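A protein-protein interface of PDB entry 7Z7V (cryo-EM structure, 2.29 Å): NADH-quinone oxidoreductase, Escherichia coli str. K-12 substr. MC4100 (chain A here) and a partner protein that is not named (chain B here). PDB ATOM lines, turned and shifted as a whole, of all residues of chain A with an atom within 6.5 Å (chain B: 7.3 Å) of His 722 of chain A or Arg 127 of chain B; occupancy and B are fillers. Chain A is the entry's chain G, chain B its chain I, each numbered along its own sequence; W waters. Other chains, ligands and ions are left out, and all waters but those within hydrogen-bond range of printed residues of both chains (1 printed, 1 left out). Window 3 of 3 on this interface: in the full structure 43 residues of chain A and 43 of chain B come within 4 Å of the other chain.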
ATOM      1  N   ARG A 716      37.934  -6.822  -3.125  1.00  0.00           N
ATOM      2  CA  ARG A 716      38.192  -7.889  -2.170  1.00  0.00           C
ATOM      3  C   ARG A 716      37.248  -9.069  -2.362  1.00  0.00           C
ATOM      4  O   ARG A 716      37.146  -9.923  -1.479  1.00  0.00           O
ATOM      5  CB  ARG A 716      38.083  -7.350  -0.745  1.00  0.00           C
ATOM      6  CG  ARG A 716      39.191  -7.790   0.170  1.00  0.00           C
ATOM      7  CD  ARG A 716      38.890  -7.393   1.597  1.00  0.00           C
ATOM      8  NE  ARG A 716      38.023  -8.362   2.256  1.00  0.00           N
ATOM      9  CZ  ARG A 716      38.432  -9.235   3.164  1.00  0.00           C
ATOM     10  NH1 ARG A 716      39.690  -9.276   3.566  1.00  0.00           N
ATOM     11  NH2 ARG A 716      37.556 -10.090   3.682  1.00  0.00           N
ATOM     12  N   ALA A 717      36.562  -9.135  -3.505  1.00  0.00           N
ATOM     13  CA  ALA A 717      35.516 -10.135  -3.697  1.00  0.00           C
ATOM     14  C   ALA A 717      36.081 -11.539  -3.858  1.00  0.00           C
ATOM     15  O   ALA A 717      35.390 -12.516  -3.551  1.00  0.00           O
ATOM     16  CB  ALA A 717      34.656  -9.773  -4.904  1.00  0.00           C
ATOM     17  N   SER A 720      36.499 -12.673  -0.240  1.00  0.00           N
ATOM     18  CA  SER A 720      35.162 -12.909   0.282  1.00  0.00           C
ATOM     19  C   SER A 720      34.191 -11.979  -0.427  1.00  0.00           C
ATOM     20  O   SER A 720      34.483 -10.798  -0.618  1.00  0.00           O
ATOM     21  CB  SER A 720      35.095 -12.683   1.795  1.00  0.00           C
ATOM     22  OG  SER A 720      33.754 -12.608   2.236  1.00  0.00           O
ATOM     23  N   VAL A 721      33.030 -12.520  -0.798  1.00  0.00           N
ATOM     24  CA  VAL A 721      32.014 -11.713  -1.459  1.00  0.00           C
ATOM     25  C   VAL A 721      31.359 -10.733  -0.489  1.00  0.00           C
ATOM     26  O   VAL A 721      30.740  -9.757  -0.922  1.00  0.00           O
ATOM     27  CB  VAL A 721      30.989 -12.642  -2.144  1.00  0.00           C
ATOM     28  CG1 VAL A 721      29.999 -13.206  -1.137  1.00  0.00           C
ATOM     29  CG2 VAL A 721      30.279 -11.926  -3.284  1.00  0.00           C
ATOM     30  N   HIS A 722      31.502 -10.948   0.817  1.00  0.00           N
ATOM     31  CA  HIS A 722      31.015  -9.998   1.807  1.00  0.00           C
ATOM     32  C   HIS A 722      32.001  -8.843   1.927  1.00  0.00           C
ATOM     33  O   HIS A 722      33.171  -9.054   2.261  1.00  0.00           O
ATOM     34  CB  HIS A 722      30.820 -10.685   3.155  1.00  0.00           C
ATOM     35  CG  HIS A 722      29.844 -11.817   3.115  1.00  0.00           C
ATOM     36  ND1 HIS A 722      28.496 -11.643   3.337  1.00  0.00           N
ATOM     37  CD2 HIS A 722      30.019 -13.136   2.868  1.00  0.00           C
ATOM     38  CE1 HIS A 722      27.882 -12.808   3.233  1.00  0.00           C
ATOM     39  NE2 HIS A 722      28.782 -13.729   2.948  1.00  0.00           N
ATOM     40  N   GLU A 723      31.531  -7.633   1.654  1.00  0.00           N
ATOM     41  CA  GLU A 723      32.395  -6.460   1.711  1.00  0.00           C
ATOM     42  C   GLU A 723      32.787  -6.180   3.155  1.00  0.00           C
ATOM     43  O   GLU A 723      31.919  -6.153   4.035  1.00  0.00           O
ATOM     44  CB  GLU A 723      31.698  -5.242   1.113  1.00  0.00           C
ATOM     45  CG  GLU A 723      31.535  -5.294  -0.391  1.00  0.00           C
ATOM     46  CD  GLU A 723      30.259  -5.996  -0.806  1.00  0.00           C
ATOM     47  OE1 GLU A 723      29.348  -6.120   0.037  1.00  0.00           O
ATOM     48  OE2 GLU A 723      30.170  -6.430  -1.970  1.00  0.00           O
ATOM     49  N   PRO A 724      34.067  -5.971   3.440  1.00  0.00           N
ATOM     50  CA  PRO A 724      34.486  -5.728   4.820  1.00  0.00           C
ATOM     51  C   PRO A 724      34.076  -4.342   5.286  1.00  0.00           C
ATOM     52  O   PRO A 724      33.665  -3.479   4.509  1.00  0.00           O
ATOM     53  CB  PRO A 724      36.006  -5.867   4.751  1.00  0.00           C
ATOM     54  CG  PRO A 724      36.336  -5.449   3.375  1.00  0.00           C
ATOM     55  CD  PRO A 724      35.197  -5.897   2.502  1.00  0.00           C
ATOM     56  N   ASN B  95      31.727  -8.890  -9.671  1.00  0.00           N
ATOM     57  CA  ASN B  95      30.833  -9.370  -8.621  1.00  0.00           C
ATOM     58  C   ASN B  95      29.415  -9.366  -9.176  1.00  0.00           C
ATOM     59  O   ASN B  95      28.726  -8.347  -9.144  1.00  0.00           O
ATOM     60  CB  ASN B  95      30.958  -8.500  -7.378  1.00  0.00           C
ATOM     61  CG  ASN B  95      30.306  -9.118  -6.158  1.00  0.00           C
ATOM     62  OD1 ASN B  95      29.655 -10.155  -6.241  1.00  0.00           O
ATOM     63  ND2 ASN B  95      30.481  -8.479  -5.014  1.00  0.00           N
ATOM     64  N   PHE B  96      28.969 -10.516  -9.675  1.00  0.00           N
ATOM     65  CA  PHE B  96      27.635 -10.606 -10.251  1.00  0.00           C
ATOM     66  C   PHE B  96      26.535 -10.688  -9.203  1.00  0.00           C
ATOM     67  O   PHE B  96      25.362 -10.544  -9.553  1.00  0.00           O
ATOM     68  CB  PHE B  96      27.544 -11.804 -11.188  1.00  0.00           C
ATOM     69  CG  PHE B  96      28.067 -11.532 -12.561  1.00  0.00           C
ATOM     70  CD1 PHE B  96      27.417 -10.650 -13.402  1.00  0.00           C
ATOM     71  CD2 PHE B  96      29.201 -12.175 -13.019  1.00  0.00           C
ATOM     72  CE1 PHE B  96      27.896 -10.408 -14.668  1.00  0.00           C
ATOM     73  CE2 PHE B  96      29.679 -11.939 -14.286  1.00  0.00           C
ATOM     74  CZ  PHE B  96      29.028 -11.054 -15.110  1.00  0.00           C
ATOM     75  N   SER B  97      26.873 -10.914  -7.934  1.00  0.00           N
ATOM     76  CA  SER B  97      25.884 -10.748  -6.879  1.00  0.00           C
ATOM     77  C   SER B  97      25.552  -9.283  -6.648  1.00  0.00           C
ATOM     78  O   SER B  97      24.510  -8.979  -6.062  1.00  0.00           O
ATOM     79  CB  SER B  97      26.375 -11.394  -5.583  1.00  0.00           C
ATOM     80  OG  SER B  97      27.195 -10.516  -4.839  1.00  0.00           O
ATOM     81  N   ARG B  98      26.408  -8.374  -7.106  1.00  0.00           N
ATOM     82  CA  ARG B  98      26.176  -6.941  -7.014  1.00  0.00           C
ATOM     83  C   ARG B  98      25.692  -6.326  -8.316  1.00  0.00           C
ATOM     84  O   ARG B  98      25.019  -5.292  -8.280  1.00  0.00           O
ATOM     85  CB  ARG B  98      27.462  -6.226  -6.588  1.00  0.00           C
ATOM     86  CG  ARG B  98      27.759  -6.308  -5.112  1.00  0.00           C
ATOM     87  CD  ARG B  98      27.082  -5.190  -4.367  1.00  0.00           C
ATOM     88  NE  ARG B  98      27.484  -5.149  -2.969  1.00  0.00           N
ATOM     89  CZ  ARG B  98      26.980  -4.313  -2.074  1.00  0.00           C
ATOM     90  NH1 ARG B  98      26.033  -3.450  -2.394  1.00  0.00           N
ATOM     91  NH2 ARG B  98      27.430  -4.354  -0.824  1.00  0.00           N
ATOM     92  N   GLU B 124      22.712 -19.357  -8.909  1.00  0.00           N
ATOM     93  CA  GLU B 124      23.863 -19.941  -8.244  1.00  0.00           C
ATOM     94  C   GLU B 124      23.469 -20.391  -6.846  1.00  0.00           C
ATOM     95  O   GLU B 124      22.555 -19.833  -6.235  1.00  0.00           O
ATOM     96  CB  GLU B 124      25.019 -18.937  -8.181  1.00  0.00           C
ATOM     97  CG  GLU B 124      26.391 -19.553  -8.026  1.00  0.00           C
ATOM     98  CD  GLU B 124      26.718 -20.557  -9.108  1.00  0.00           C
ATOM     99  OE1 GLU B 124      27.131 -20.136 -10.208  1.00  0.00           O
ATOM    100  OE2 GLU B 124      26.570 -21.771  -8.856  1.00  0.00           O
ATOM    101  N   TYR B 125      24.179 -21.398  -6.342  1.00  0.00           N
ATOM    102  CA  TYR B 125      23.933 -21.915  -5.003  1.00  0.00           C
ATOM    103  C   TYR B 125      24.676 -21.135  -3.927  1.00  0.00           C
ATOM    104  O   TYR B 125      24.100 -20.831  -2.879  1.00  0.00           O
ATOM    105  CB  TYR B 125      24.314 -23.393  -4.939  1.00  0.00           C
ATOM    106  CG  TYR B 125      23.446 -24.261  -5.811  1.00  0.00           C
ATOM    107  CD1 TYR B 125      22.092 -24.392  -5.553  1.00  0.00           C
ATOM    108  CD2 TYR B 125      23.975 -24.937  -6.899  1.00  0.00           C
ATOM    109  CE1 TYR B 125      21.289 -25.177  -6.344  1.00  0.00           C
ATOM    110  CE2 TYR B 125      23.179 -25.725  -7.699  1.00  0.00           C
ATOM    111  CZ  TYR B 125      21.836 -25.842  -7.416  1.00  0.00           C
ATOM    112  OH  TYR B 125      21.033 -26.625  -8.205  1.00  0.00           O
ATOM    113  N   LYS B 126      25.940 -20.804  -4.160  1.00  0.00           N
ATOM    114  CA  LYS B 126      26.739 -20.036  -3.218  1.00  0.00           C
ATOM    115  C   LYS B 126      27.049 -18.672  -3.812  1.00  0.00           C
ATOM    116  O   LYS B 126      27.356 -18.559  -5.000  1.00  0.00           O
ATOM    117  CB  LYS B 126      28.039 -20.761  -2.871  1.00  0.00           C
ATOM    118  CG  LYS B 126      27.852 -22.203  -2.444  1.00  0.00           C
ATOM    119  CD  LYS B 126      27.649 -22.299  -0.948  1.00  0.00           C
ATOM    120  CE  LYS B 126      26.683 -23.413  -0.592  1.00  0.00           C
ATOM    121  NZ  LYS B 126      27.395 -24.691  -0.308  1.00  0.00           N
ATOM    122  N   ARG B 127      26.964 -17.638  -2.975  1.00  0.00           N
ATOM    123  CA  ARG B 127      27.180 -16.277  -3.451  1.00  0.00           C
ATOM    124  C   ARG B 127      28.632 -16.036  -3.851  1.00  0.00           C
ATOM    125  O   ARG B 127      28.896 -15.224  -4.744  1.00  0.00           O
ATOM    126  CB  ARG B 127      26.745 -15.276  -2.384  1.00  0.00           C
ATOM    127  CG  ARG B 127      26.760 -13.842  -2.858  1.00  0.00           C
ATOM    128  CD  ARG B 127      25.635 -13.045  -2.284  1.00  0.00           C
ATOM    129  NE  ARG B 127      25.920 -12.560  -0.940  1.00  0.00           N
ATOM    130  CZ  ARG B 127      26.676 -11.507  -0.661  1.00  0.00           C
ATOM    131  NH1 ARG B 127      27.285 -10.821  -1.611  1.00  0.00           N
ATOM    132  NH2 ARG B 127      26.819 -11.131   0.604  1.00  0.00           N
ATOM    133  N   GLN B 128      29.575 -16.739  -3.220  1.00  0.00           N
ATOM    134  CA  GLN B 128      30.984 -16.604  -3.581  1.00  0.00           C
ATOM    135  C   GLN B 128      31.244 -17.049  -5.015  1.00  0.00           C
ATOM    136  O   GLN B 128      32.147 -16.527  -5.674  1.00  0.00           O
ATOM    137  CB  GLN B 128      31.849 -17.405  -2.608  1.00  0.00           C
ATOM    138  CG  GLN B 128      33.343 -17.146  -2.719  1.00  0.00           C
ATOM    139  CD  GLN B 128      33.707 -15.701  -2.469  1.00  0.00           C
ATOM    140  OE1 GLN B 128      33.337 -15.125  -1.450  1.00  0.00           O
ATOM    141  NE2 GLN B 128      34.436 -15.105  -3.399  1.00  0.00           N
ATOM    142  N   ASP B 129      30.444 -17.982  -5.525  1.00  0.00           N
ATOM    143  CA  ASP B 129      30.577 -18.448  -6.898  1.00  0.00           C
ATOM    144  C   ASP B 129      30.019 -17.466  -7.917  1.00  0.00           C
ATOM    145  O   ASP B 129      30.182 -17.692  -9.119  1.00  0.00           O
ATOM    146  CB  ASP B 129      29.890 -19.803  -7.048  1.00  0.00           C
ATOM    147  CG  ASP B 129      30.632 -20.908  -6.332  1.00  0.00           C
ATOM    148  OD1 ASP B 129      31.866 -20.799  -6.188  1.00  0.00           O
ATOM    149  OD2 ASP B 129      29.981 -21.874  -5.890  1.00  0.00           O
ATOM    150  N   LEU B 130      29.366 -16.395  -7.476  1.00  0.00           N
ATOM    151  CA  LEU B 130      28.931 -15.336  -8.373  1.00  0.00           C
ATOM    152  C   LEU B 130      30.035 -14.333  -8.680  1.00  0.00           C
ATOM    153  O   LEU B 130      29.814 -13.423  -9.481  1.00  0.00           O
ATOM    154  CB  LEU B 130      27.720 -14.610  -7.783  1.00  0.00           C
ATOM    155  CG  LEU B 130      26.381 -15.327  -7.959  1.00  0.00           C
ATOM    156  CD1 LEU B 130      25.264 -14.558  -7.278  1.00  0.00           C
ATOM    157  CD2 LEU B 130      26.078 -15.543  -9.427  1.00  0.00           C
ATOM    158  N   VAL B 131      31.205 -14.470  -8.067  1.00  0.00           N
ATOM    159  CA  VAL B 131      32.363 -13.653  -8.410  1.00  0.00           C
ATOM    160  C   VAL B 131      33.052 -14.319  -9.595  1.00  0.00           C
ATOM    161  O   VAL B 131      33.703 -15.354  -9.447  1.00  0.00           O
ATOM    162  CB  VAL B 131      33.317 -13.495  -7.222  1.00  0.00           C
ATOM    163  CG1 VAL B 131      34.480 -12.600  -7.596  1.00  0.00           C
ATOM    164  CG2 VAL B 131      32.579 -12.930  -6.030  1.00  0.00           C
HETATM  165  O   HOH W   1      27.231  -7.802   0.165  1.00  0.00           O
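Of the 12 printed residues of chain B, 6 touch a printed residue of chain A.
Printed residues of chain B that touch a printed residue of chain A: Asn 95, Ser 97, Arg 98, Arg 127, Gln 128 and Val 131.
The side-chain hydroxyl of Ser 720 of chain A is in hydrogen-bond range of the backbone NH of His 722 of chain A (3.1 Å).
The side-chain amide oxygen (OD1) of Asn 95 of chain B sits at hydrogen-bond distance from the side-chain hydroxyl (OG) of Ser 97 of chain B, at 2.9 Å.
OG of Ser 97 of chain B is in hydrogen-bond range of NH1 of Arg 127 of chain B (3.2 Å).
Printed residues of chain B within 4 Å of Ser 720 of chain A: Gln 128 (3.4 Å).
Of the printed residues of chain B, His 722 of chain A touches Arg 127.
Printed residues of chain A within 4 Å of Arg 98 of chain B: Glu 723.
Of the printed residues of chain A, Gln 128 of chain B touches Ala 717, Ser 720 and Val 721.
The nearest residue of chain A that does not touch Arg 127 of chain B is Glu 723 of chain A (5.3 Å).
The nearest printed residue of chain A that does not touch Val 131 of chain B is Ser 720 of chain A (5.9 Å).
Water W1 lies within hydrogen-bond range of OE1 of Glu 723 of chain A (2.7 Å) and NH2 of Arg 127 of chain B (3.4 Å).
Among the printed residues, merely in contact across the chains: Ala 717 of chain A with Val 131 of chain B (3.8 Å), Ser 720 of chain A with Gln 128 of chain B (3.4 Å), Val 721 of chain A with Asn 95 of chain B (3.5 Å), Val 721 of chain A with Ser 97 of chain B (3.7 Å), Val 721 of chain A with Arg 127 of chain B (3.6 Å), Val 721 of chain A with Val 131 of chain B (3.7 Å) and Glu 723 of chain A with Asn 95 of chain B (3.7 Å).
The side-chain amide nitrogen (NE2) of Gln 128 of chain B lies within hydrogen-bond range of the backbone carbonyl oxygen (O) of Ala 717 of chain A (2.8 Å).
The side-chain amide oxygen (OE1) of Gln 128 of chain B lies within hydrogen-bond range of the backbone NH (N) of Val 721 of chain A (2.7 Å).
A ring nitrogen (ND1) of His 722 of chain A is in hydrogen-bond range of the guanidinium group of Arg 127 of chain B (3.2 Å).
NH2 of Arg 98 of chain B lies within salt-bridge range of OE1 of Glu 723 of chain A (2.7 Å).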
